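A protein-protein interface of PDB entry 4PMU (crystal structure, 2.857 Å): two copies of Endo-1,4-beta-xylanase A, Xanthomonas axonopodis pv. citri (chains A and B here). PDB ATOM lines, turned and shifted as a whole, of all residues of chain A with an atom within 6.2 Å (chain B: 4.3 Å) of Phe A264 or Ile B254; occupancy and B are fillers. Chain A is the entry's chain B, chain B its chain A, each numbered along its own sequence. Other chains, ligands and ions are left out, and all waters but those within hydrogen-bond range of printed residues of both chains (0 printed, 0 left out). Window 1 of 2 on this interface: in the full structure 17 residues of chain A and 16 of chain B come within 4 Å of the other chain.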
ATOM      1  N   GLY A 258     -11.349  15.126 -15.773  1.00  0.00           N
ATOM      2  CA  GLY A 258     -12.318  16.216 -15.855  1.00  0.00           C
ATOM      3  C   GLY A 258     -13.437  15.969 -16.848  1.00  0.00           C
ATOM      4  O   GLY A 258     -14.611  16.127 -16.521  1.00  0.00           O
ATOM      5  N   MET A 259     -13.066  15.566 -18.059  1.00  0.00           N
ATOM      6  CA  MET A 259     -14.028  15.338 -19.139  1.00  0.00           C
ATOM      7  C   MET A 259     -14.796  14.013 -19.000  1.00  0.00           C
ATOM      8  O   MET A 259     -15.720  13.732 -19.772  1.00  0.00           O
ATOM      9  CB  MET A 259     -13.331  15.424 -20.501  1.00  0.00           C
ATOM     10  CG  MET A 259     -12.433  16.641 -20.690  1.00  0.00           C
ATOM     11  SD  MET A 259     -13.193  18.232 -20.294  1.00  0.00           S
ATOM     12  CE  MET A 259     -14.543  18.298 -21.473  1.00  0.00           C
ATOM     13  N   ALA A 260     -14.419  13.210 -18.007  1.00  0.00           N
ATOM     14  CA  ALA A 260     -15.128  11.972 -17.693  1.00  0.00           C
ATOM     15  C   ALA A 260     -16.404  12.223 -16.873  1.00  0.00           C
ATOM     16  O   ALA A 260     -17.044  11.279 -16.401  1.00  0.00           O
ATOM     17  CB  ALA A 260     -14.202  11.006 -16.967  1.00  0.00           C
ATOM     18  N   HIS A 261     -16.763  13.497 -16.716  1.00  0.00           N
ATOM     19  CA  HIS A 261     -17.913  13.909 -15.908  1.00  0.00           C
ATOM     20  C   HIS A 261     -19.213  13.635 -16.656  1.00  0.00           C
ATOM     21  O   HIS A 261     -19.295  13.830 -17.872  1.00  0.00           O
ATOM     22  CB  HIS A 261     -17.802  15.395 -15.563  1.00  0.00           C
ATOM     23  CG  HIS A 261     -18.672  15.827 -14.422  1.00  0.00           C
ATOM     24  ND1 HIS A 261     -20.029  16.029 -14.551  1.00  0.00           N
ATOM     25  CD2 HIS A 261     -18.369  16.126 -13.136  1.00  0.00           C
ATOM     26  CE1 HIS A 261     -20.528  16.422 -13.393  1.00  0.00           C
ATOM     27  NE2 HIS A 261     -19.542  16.491 -12.517  1.00  0.00           N
ATOM     28  N   LYS A 262     -20.227  13.191 -15.916  1.00  0.00           N
ATOM     29  CA  LYS A 262     -21.528  12.823 -16.482  1.00  0.00           C
ATOM     30  C   LYS A 262     -22.087  13.923 -17.376  1.00  0.00           C
ATOM     31  O   LYS A 262     -22.802  13.645 -18.343  1.00  0.00           O
ATOM     32  CB  LYS A 262     -22.547  12.503 -15.371  1.00  0.00           C
ATOM     33  CG  LYS A 262     -21.969  11.929 -14.077  1.00  0.00           C
ATOM     34  CD  LYS A 262     -21.267  10.584 -14.275  1.00  0.00           C
ATOM     35  CE  LYS A 262     -20.177  10.362 -13.233  1.00  0.00           C
ATOM     36  NZ  LYS A 262     -19.119  11.412 -13.309  1.00  0.00           N
ATOM     37  N   GLN A 263     -21.745  15.167 -17.051  1.00  0.00           N
ATOM     38  CA  GLN A 263     -22.291  16.330 -17.746  1.00  0.00           C
ATOM     39  C   GLN A 263     -21.884  16.435 -19.213  1.00  0.00           C
ATOM     40  O   GLN A 263     -22.651  16.944 -20.029  1.00  0.00           O
ATOM     41  CB  GLN A 263     -21.969  17.629 -16.995  1.00  0.00           C
ATOM     42  CG  GLN A 263     -20.522  18.085 -17.072  1.00  0.00           C
ATOM     43  CD  GLN A 263     -20.242  19.256 -16.157  1.00  0.00           C
ATOM     44  OE1 GLN A 263     -21.133  20.050 -15.855  1.00  0.00           O
ATOM     45  NE2 GLN A 263     -18.997  19.369 -15.709  1.00  0.00           N
ATOM     46  N   PHE A 264     -20.691  15.950 -19.549  1.00  0.00           N
ATOM     47  CA  PHE A 264     -20.228  15.985 -20.935  1.00  0.00           C
ATOM     48  C   PHE A 264     -20.812  14.836 -21.774  1.00  0.00           C
ATOM     49  O   PHE A 264     -20.559  14.736 -22.979  1.00  0.00           O
ATOM     50  CB  PHE A 264     -18.692  16.043 -21.002  1.00  0.00           C
ATOM     51  CG  PHE A 264     -18.096  17.220 -20.265  1.00  0.00           C
ATOM     52  CD1 PHE A 264     -18.276  18.523 -20.732  1.00  0.00           C
ATOM     53  CD2 PHE A 264     -17.354  17.028 -19.102  1.00  0.00           C
ATOM     54  CE1 PHE A 264     -17.732  19.606 -20.051  1.00  0.00           C
ATOM     55  CE2 PHE A 264     -16.808  18.108 -18.418  1.00  0.00           C
ATOM     56  CZ  PHE A 264     -16.996  19.398 -18.892  1.00  0.00           C
ATOM     57  N   GLN A 265     -21.605  13.984 -21.124  1.00  0.00           N
ATOM     58  CA  GLN A 265     -22.358  12.930 -21.807  1.00  0.00           C
ATOM     59  C   GLN A 265     -23.781  13.387 -22.138  1.00  0.00           C
ATOM     60  O   GLN A 265     -24.485  12.733 -22.911  1.00  0.00           O
ATOM     61  CB  GLN A 265     -22.400  11.641 -20.969  1.00  0.00           C
ATOM     62  CG  GLN A 265     -21.047  10.991 -20.696  1.00  0.00           C
ATOM     63  CD  GLN A 265     -20.302  10.566 -21.955  1.00  0.00           C
ATOM     64  OE1 GLN A 265     -19.072  10.558 -21.981  1.00  0.00           O
ATOM     65  NE2 GLN A 265     -21.041  10.209 -23.003  1.00  0.00           N
ATOM     66  N   LEU A 266     -24.197  14.507 -21.550  1.00  0.00           N
ATOM     67  CA  LEU A 266     -25.526  15.067 -21.794  1.00  0.00           C
ATOM     68  C   LEU A 266     -25.670  15.556 -23.239  1.00  0.00           C
ATOM     69  O   LEU A 266     -24.698  16.033 -23.829  1.00  0.00           O
ATOM     70  CB  LEU A 266     -25.832  16.192 -20.800  1.00  0.00           C
ATOM     71  CG  LEU A 266     -25.944  15.820 -19.315  1.00  0.00           C
ATOM     72  CD1 LEU A 266     -25.842  17.072 -18.454  1.00  0.00           C
ATOM     73  CD2 LEU A 266     -27.221  15.043 -19.003  1.00  0.00           C
ATOM     74  N   PHE A 269     -23.843  18.541 -24.928  1.00  0.00           N
ATOM     75  CA  PHE A 269     -22.389  18.447 -25.020  1.00  0.00           C
ATOM     76  C   PHE A 269     -21.944  17.391 -26.020  1.00  0.00           C
ATOM     77  O   PHE A 269     -21.036  17.639 -26.812  1.00  0.00           O
ATOM     78  CB  PHE A 269     -21.750  18.211 -23.645  1.00  0.00           C
ATOM     79  CG  PHE A 269     -21.692  19.444 -22.788  1.00  0.00           C
ATOM     80  CD1 PHE A 269     -20.926  20.541 -23.172  1.00  0.00           C
ATOM     81  CD2 PHE A 269     -22.406  19.515 -21.602  1.00  0.00           C
ATOM     82  CE1 PHE A 269     -20.878  21.682 -22.391  1.00  0.00           C
ATOM     83  CE2 PHE A 269     -22.360  20.651 -20.813  1.00  0.00           C
ATOM     84  CZ  PHE A 269     -21.593  21.733 -21.208  1.00  0.00           C
ATOM     85  N   LYS A 270     -22.590  16.227 -25.993  1.00  0.00           N
ATOM     86  CA  LYS A 270     -22.313  15.173 -26.969  1.00  0.00           C
ATOM     87  C   LYS A 270     -22.501  15.721 -28.386  1.00  0.00           C
ATOM     88  O   LYS A 270     -21.707  15.436 -29.282  1.00  0.00           O
ATOM     89  CB  LYS A 270     -23.194  13.940 -26.721  1.00  0.00           C
ATOM     90  CG  LYS A 270     -22.720  12.691 -27.453  1.00  0.00           C
ATOM     91  CD  LYS A 270     -23.200  11.413 -26.779  1.00  0.00           C
ATOM     92  CE  LYS A 270     -23.014  10.191 -27.679  1.00  0.00           C
ATOM     93  NZ  LYS A 270     -21.593   9.815 -27.945  1.00  0.00           N
ATOM     94  N   LEU A 273     -19.235  17.955 -28.813  1.00  0.00           N
ATOM     95  CA  LEU A 273     -17.957  17.267 -28.665  1.00  0.00           C
ATOM     96  C   LEU A 273     -17.797  16.073 -29.603  1.00  0.00           C
ATOM     97  O   LEU A 273     -16.673  15.657 -29.898  1.00  0.00           O
ATOM     98  CB  LEU A 273     -17.775  16.794 -27.220  1.00  0.00           C
ATOM     99  CG  LEU A 273     -17.795  17.804 -26.072  1.00  0.00           C
ATOM    100  CD1 LEU A 273     -17.958  17.076 -24.745  1.00  0.00           C
ATOM    101  CD2 LEU A 273     -16.544  18.670 -26.067  1.00  0.00           C
ATOM    102  N   VAL A 326     -12.733  12.308 -23.351  1.00  0.00           N
ATOM    103  CA  VAL A 326     -14.186  12.156 -23.221  1.00  0.00           C
ATOM    104  C   VAL A 326     -14.618  10.800 -23.770  1.00  0.00           C
ATOM    105  O   VAL A 326     -14.448  10.539 -24.965  1.00  0.00           O
ATOM    106  CB  VAL A 326     -14.972  13.263 -23.961  1.00  0.00           C
ATOM    107  CG1 VAL A 326     -16.419  13.289 -23.491  1.00  0.00           C
ATOM    108  CG2 VAL A 326     -14.324  14.630 -23.782  1.00  0.00           C
ATOM    109  N   PRO A 327     -15.167   9.929 -22.898  1.00  0.00           N
ATOM    110  CA  PRO A 327     -15.638   8.593 -23.298  1.00  0.00           C
ATOM    111  C   PRO A 327     -16.789   8.602 -24.307  1.00  0.00           C
ATOM    112  O   PRO A 327     -17.562   9.561 -24.366  1.00  0.00           O
ATOM    113  CB  PRO A 327     -16.099   7.959 -21.973  1.00  0.00           C
ATOM    114  CG  PRO A 327     -16.251   9.089 -21.019  1.00  0.00           C
ATOM    115  CD  PRO A 327     -15.256  10.125 -21.439  1.00  0.00           C
ATOM    116  N   LEU B 248     -17.093  26.432 -25.915  1.00  0.00           N
ATOM    117  CA  LEU B 248     -17.489  25.365 -24.985  1.00  0.00           C
ATOM    118  C   LEU B 248     -18.697  25.723 -24.120  1.00  0.00           C
ATOM    119  O   LEU B 248     -19.684  24.989 -24.110  1.00  0.00           O
ATOM    120  CB  LEU B 248     -16.318  24.896 -24.106  1.00  0.00           C
ATOM    121  CG  LEU B 248     -16.637  23.864 -23.019  1.00  0.00           C
ATOM    122  CD1 LEU B 248     -17.064  22.531 -23.613  1.00  0.00           C
ATOM    123  CD2 LEU B 248     -15.437  23.675 -22.109  1.00  0.00           C
ATOM    124  N   GLY B 252     -23.338  24.412 -23.599  1.00  0.00           N
ATOM    125  CA  GLY B 252     -24.079  23.822 -22.483  1.00  0.00           C
ATOM    126  C   GLY B 252     -23.606  24.376 -21.149  1.00  0.00           C
ATOM    127  O   GLY B 252     -22.516  24.949 -21.063  1.00  0.00           O
ATOM    128  N   GLN B 253     -24.423  24.213 -20.110  1.00  0.00           N
ATOM    129  CA  GLN B 253     -24.070  24.695 -18.772  1.00  0.00           C
ATOM    130  C   GLN B 253     -23.136  23.698 -18.095  1.00  0.00           C
ATOM    131  O   GLN B 253     -23.386  22.493 -18.125  1.00  0.00           O
ATOM    132  CB  GLN B 253     -25.321  24.932 -17.919  1.00  0.00           C
ATOM    133  CG  GLN B 253     -25.112  25.898 -16.758  1.00  0.00           C
ATOM    134  CD  GLN B 253     -26.353  26.096 -15.898  1.00  0.00           C
ATOM    135  OE1 GLN B 253     -27.481  26.113 -16.394  1.00  0.00           O
ATOM    136  NE2 GLN B 253     -26.145  26.262 -14.599  1.00  0.00           N
ATOM    137  N   ILE B 254     -22.060  24.206 -17.500  1.00  0.00           N
ATOM    138  CA  ILE B 254     -21.085  23.359 -16.825  1.00  0.00           C
ATOM    139  C   ILE B 254     -21.134  23.565 -15.312  1.00  0.00           C
ATOM    140  O   ILE B 254     -21.181  24.701 -14.823  1.00  0.00           O
ATOM    141  CB  ILE B 254     -19.650  23.601 -17.355  1.00  0.00           C
ATOM    142  CG1 ILE B 254     -19.571  23.268 -18.846  1.00  0.00           C
ATOM    143  CG2 ILE B 254     -18.634  22.770 -16.580  1.00  0.00           C
ATOM    144  CD1 ILE B 254     -18.195  23.408 -19.462  1.00  0.00           C
ATOM    145  N   ILE B 255     -21.136  22.457 -14.576  1.00  0.00           N
ATOM    146  CA  ILE B 255     -20.989  22.489 -13.123  1.00  0.00           C
ATOM    147  C   ILE B 255     -19.663  21.837 -12.710  1.00  0.00           C
ATOM    148  O   ILE B 255     -18.941  21.290 -13.552  1.00  0.00           O
ATOM    149  CB  ILE B 255     -22.187  21.832 -12.400  1.00  0.00           C
ATOM    150  CG1 ILE B 255     -22.246  20.325 -12.688  1.00  0.00           C
ATOM    151  CG2 ILE B 255     -23.486  22.519 -12.804  1.00  0.00           C
ATOM    152  CD1 ILE B 255     -22.939  19.508 -11.615  1.00  0.00           C
ATOM    153  N   MET B 259     -13.321  22.514 -14.895  1.00  0.00           N
ATOM    154  CA  MET B 259     -12.872  23.552 -15.822  1.00  0.00           C
ATOM    155  C   MET B 259     -11.941  24.549 -15.142  1.00  0.00           C
ATOM    156  O   MET B 259     -11.226  25.302 -15.810  1.00  0.00           O
ATOM    157  CB  MET B 259     -14.055  24.279 -16.475  1.00  0.00           C
ATOM    158  CG  MET B 259     -14.810  23.474 -17.530  1.00  0.00           C
ATOM    159  SD  MET B 259     -13.803  22.471 -18.651  1.00  0.00           S
ATOM    160  CE  MET B 259     -12.847  23.718 -19.514  1.00  0.00           C
ATOM    161  N   TYR B 324     -16.217  31.836 -13.893  1.00  0.00           N
ATOM    162  CA  TYR B 324     -16.776  30.486 -13.844  1.00  0.00           C
ATOM    163  C   TYR B 324     -17.378  30.062 -15.187  1.00  0.00           C
ATOM    164  O   TYR B 324     -18.008  30.877 -15.860  1.00  0.00           O
ATOM    165  CB  TYR B 324     -17.805  30.346 -12.718  1.00  0.00           C
ATOM    166  CG  TYR B 324     -18.169  28.909 -12.447  1.00  0.00           C
ATOM    167  CD1 TYR B 324     -17.341  28.091 -11.670  1.00  0.00           C
ATOM    168  CD2 TYR B 324     -19.324  28.351 -12.993  1.00  0.00           C
ATOM    169  CE1 TYR B 324     -17.662  26.762 -11.436  1.00  0.00           C
ATOM    170  CE2 TYR B 324     -19.655  27.025 -12.765  1.00  0.00           C
ATOM    171  CZ  TYR B 324     -18.824  26.237 -11.988  1.00  0.00           C
ATOM    172  OH  TYR B 324     -19.164  24.923 -11.766  1.00  0.00           O
ATOM    173  N   PRO B 325     -17.178  28.788 -15.589  1.00  0.00           N
ATOM    174  CA  PRO B 325     -16.393  27.729 -14.936  1.00  0.00           C
ATOM    175  C   PRO B 325     -14.887  27.837 -15.148  1.00  0.00           C
ATOM    176  O   PRO B 325     -14.130  27.098 -14.515  1.00  0.00           O
ATOM    177  CB  PRO B 325     -16.921  26.452 -15.591  1.00  0.00           C
ATOM    178  CG  PRO B 325     -17.350  26.888 -16.948  1.00  0.00           C
ATOM    179  CD  PRO B 325     -17.909  28.272 -16.763  1.00  0.00           C
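The backbone NH (N) of Ile B255 is in hydrogen-bond range of the side-chain amide oxygen (OE1) of Gln A263, at 2.7 Å.
A ring nitrogen (ND1) of His A261 lies close to the backbone NH (N) of Gln A263 (3.2 Å).
Gln A263 touches Ile B254.
Phe A264 touches Ile B254.
Phe A269 touches Leu B248 (CE1 to O, 3.9 Å).
Phe A269 touches Gly B252 (CZ to C, 3.3 Å).
CE2 of Phe A269 touches O of Gln B253 (3.4 Å).
Phe A269 touches Ile B254 (CZ to CG1, 3.5 Å).
Phe A264 touches just one residue of chain B: Ile B254 (3.9 Å).
Ile B254 touches just these residues of chain A: Gln A263, Phe A264 and Phe A269.
Of the printed residues of chain A, Leu B248 touches Phe A269 (3.9 Å).
Of the printed residues of chain B, Gln A263 touches Ile B254 (3.4 Å) and Ile B255 (2.7 Å).
Of the printed residues of chain A, Gln B253 touches Phe A269.
Of the printed residues of chain A, Gly B252 touches Phe A269.
Printed residues of chain B within 4 Å of Phe A269: Leu B248, Gly B252, Gln B253 and Ile B254.
Leu A273 touches none of the printed residues of chain B.
Met B259 touches none of the printed residues of chain A.
Of the 8 printed residues of chain B, 5 touch a printed residue of chain A.
Hydrophobic or aromatic side chains of chain B that line the printed part of chain A: Ile B254 and Ile B255.
Of the 14 printed residues of chain A, 3 touch a printed residue of chain B.
Printed residues of chain A that touch a printed residue of chain B: Gln A263, Phe A264 and Phe A269.
Hydrophobic or aromatic side chains of chain A within 4 Å of the printed part of chain B: Phe A264 and Phe A269.
Among the printed residues, 7 pairs touch across the chains.
Among the printed residues, no Asp or Glu carboxylate lies within 4 Å of a Lys or Arg side-chain nitrogen of the other chain.
Position printed for both chains: 259.
Of the 7 pairs that touch across the chains among the printed residues, none has its exchanged pair printed and touching as well.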
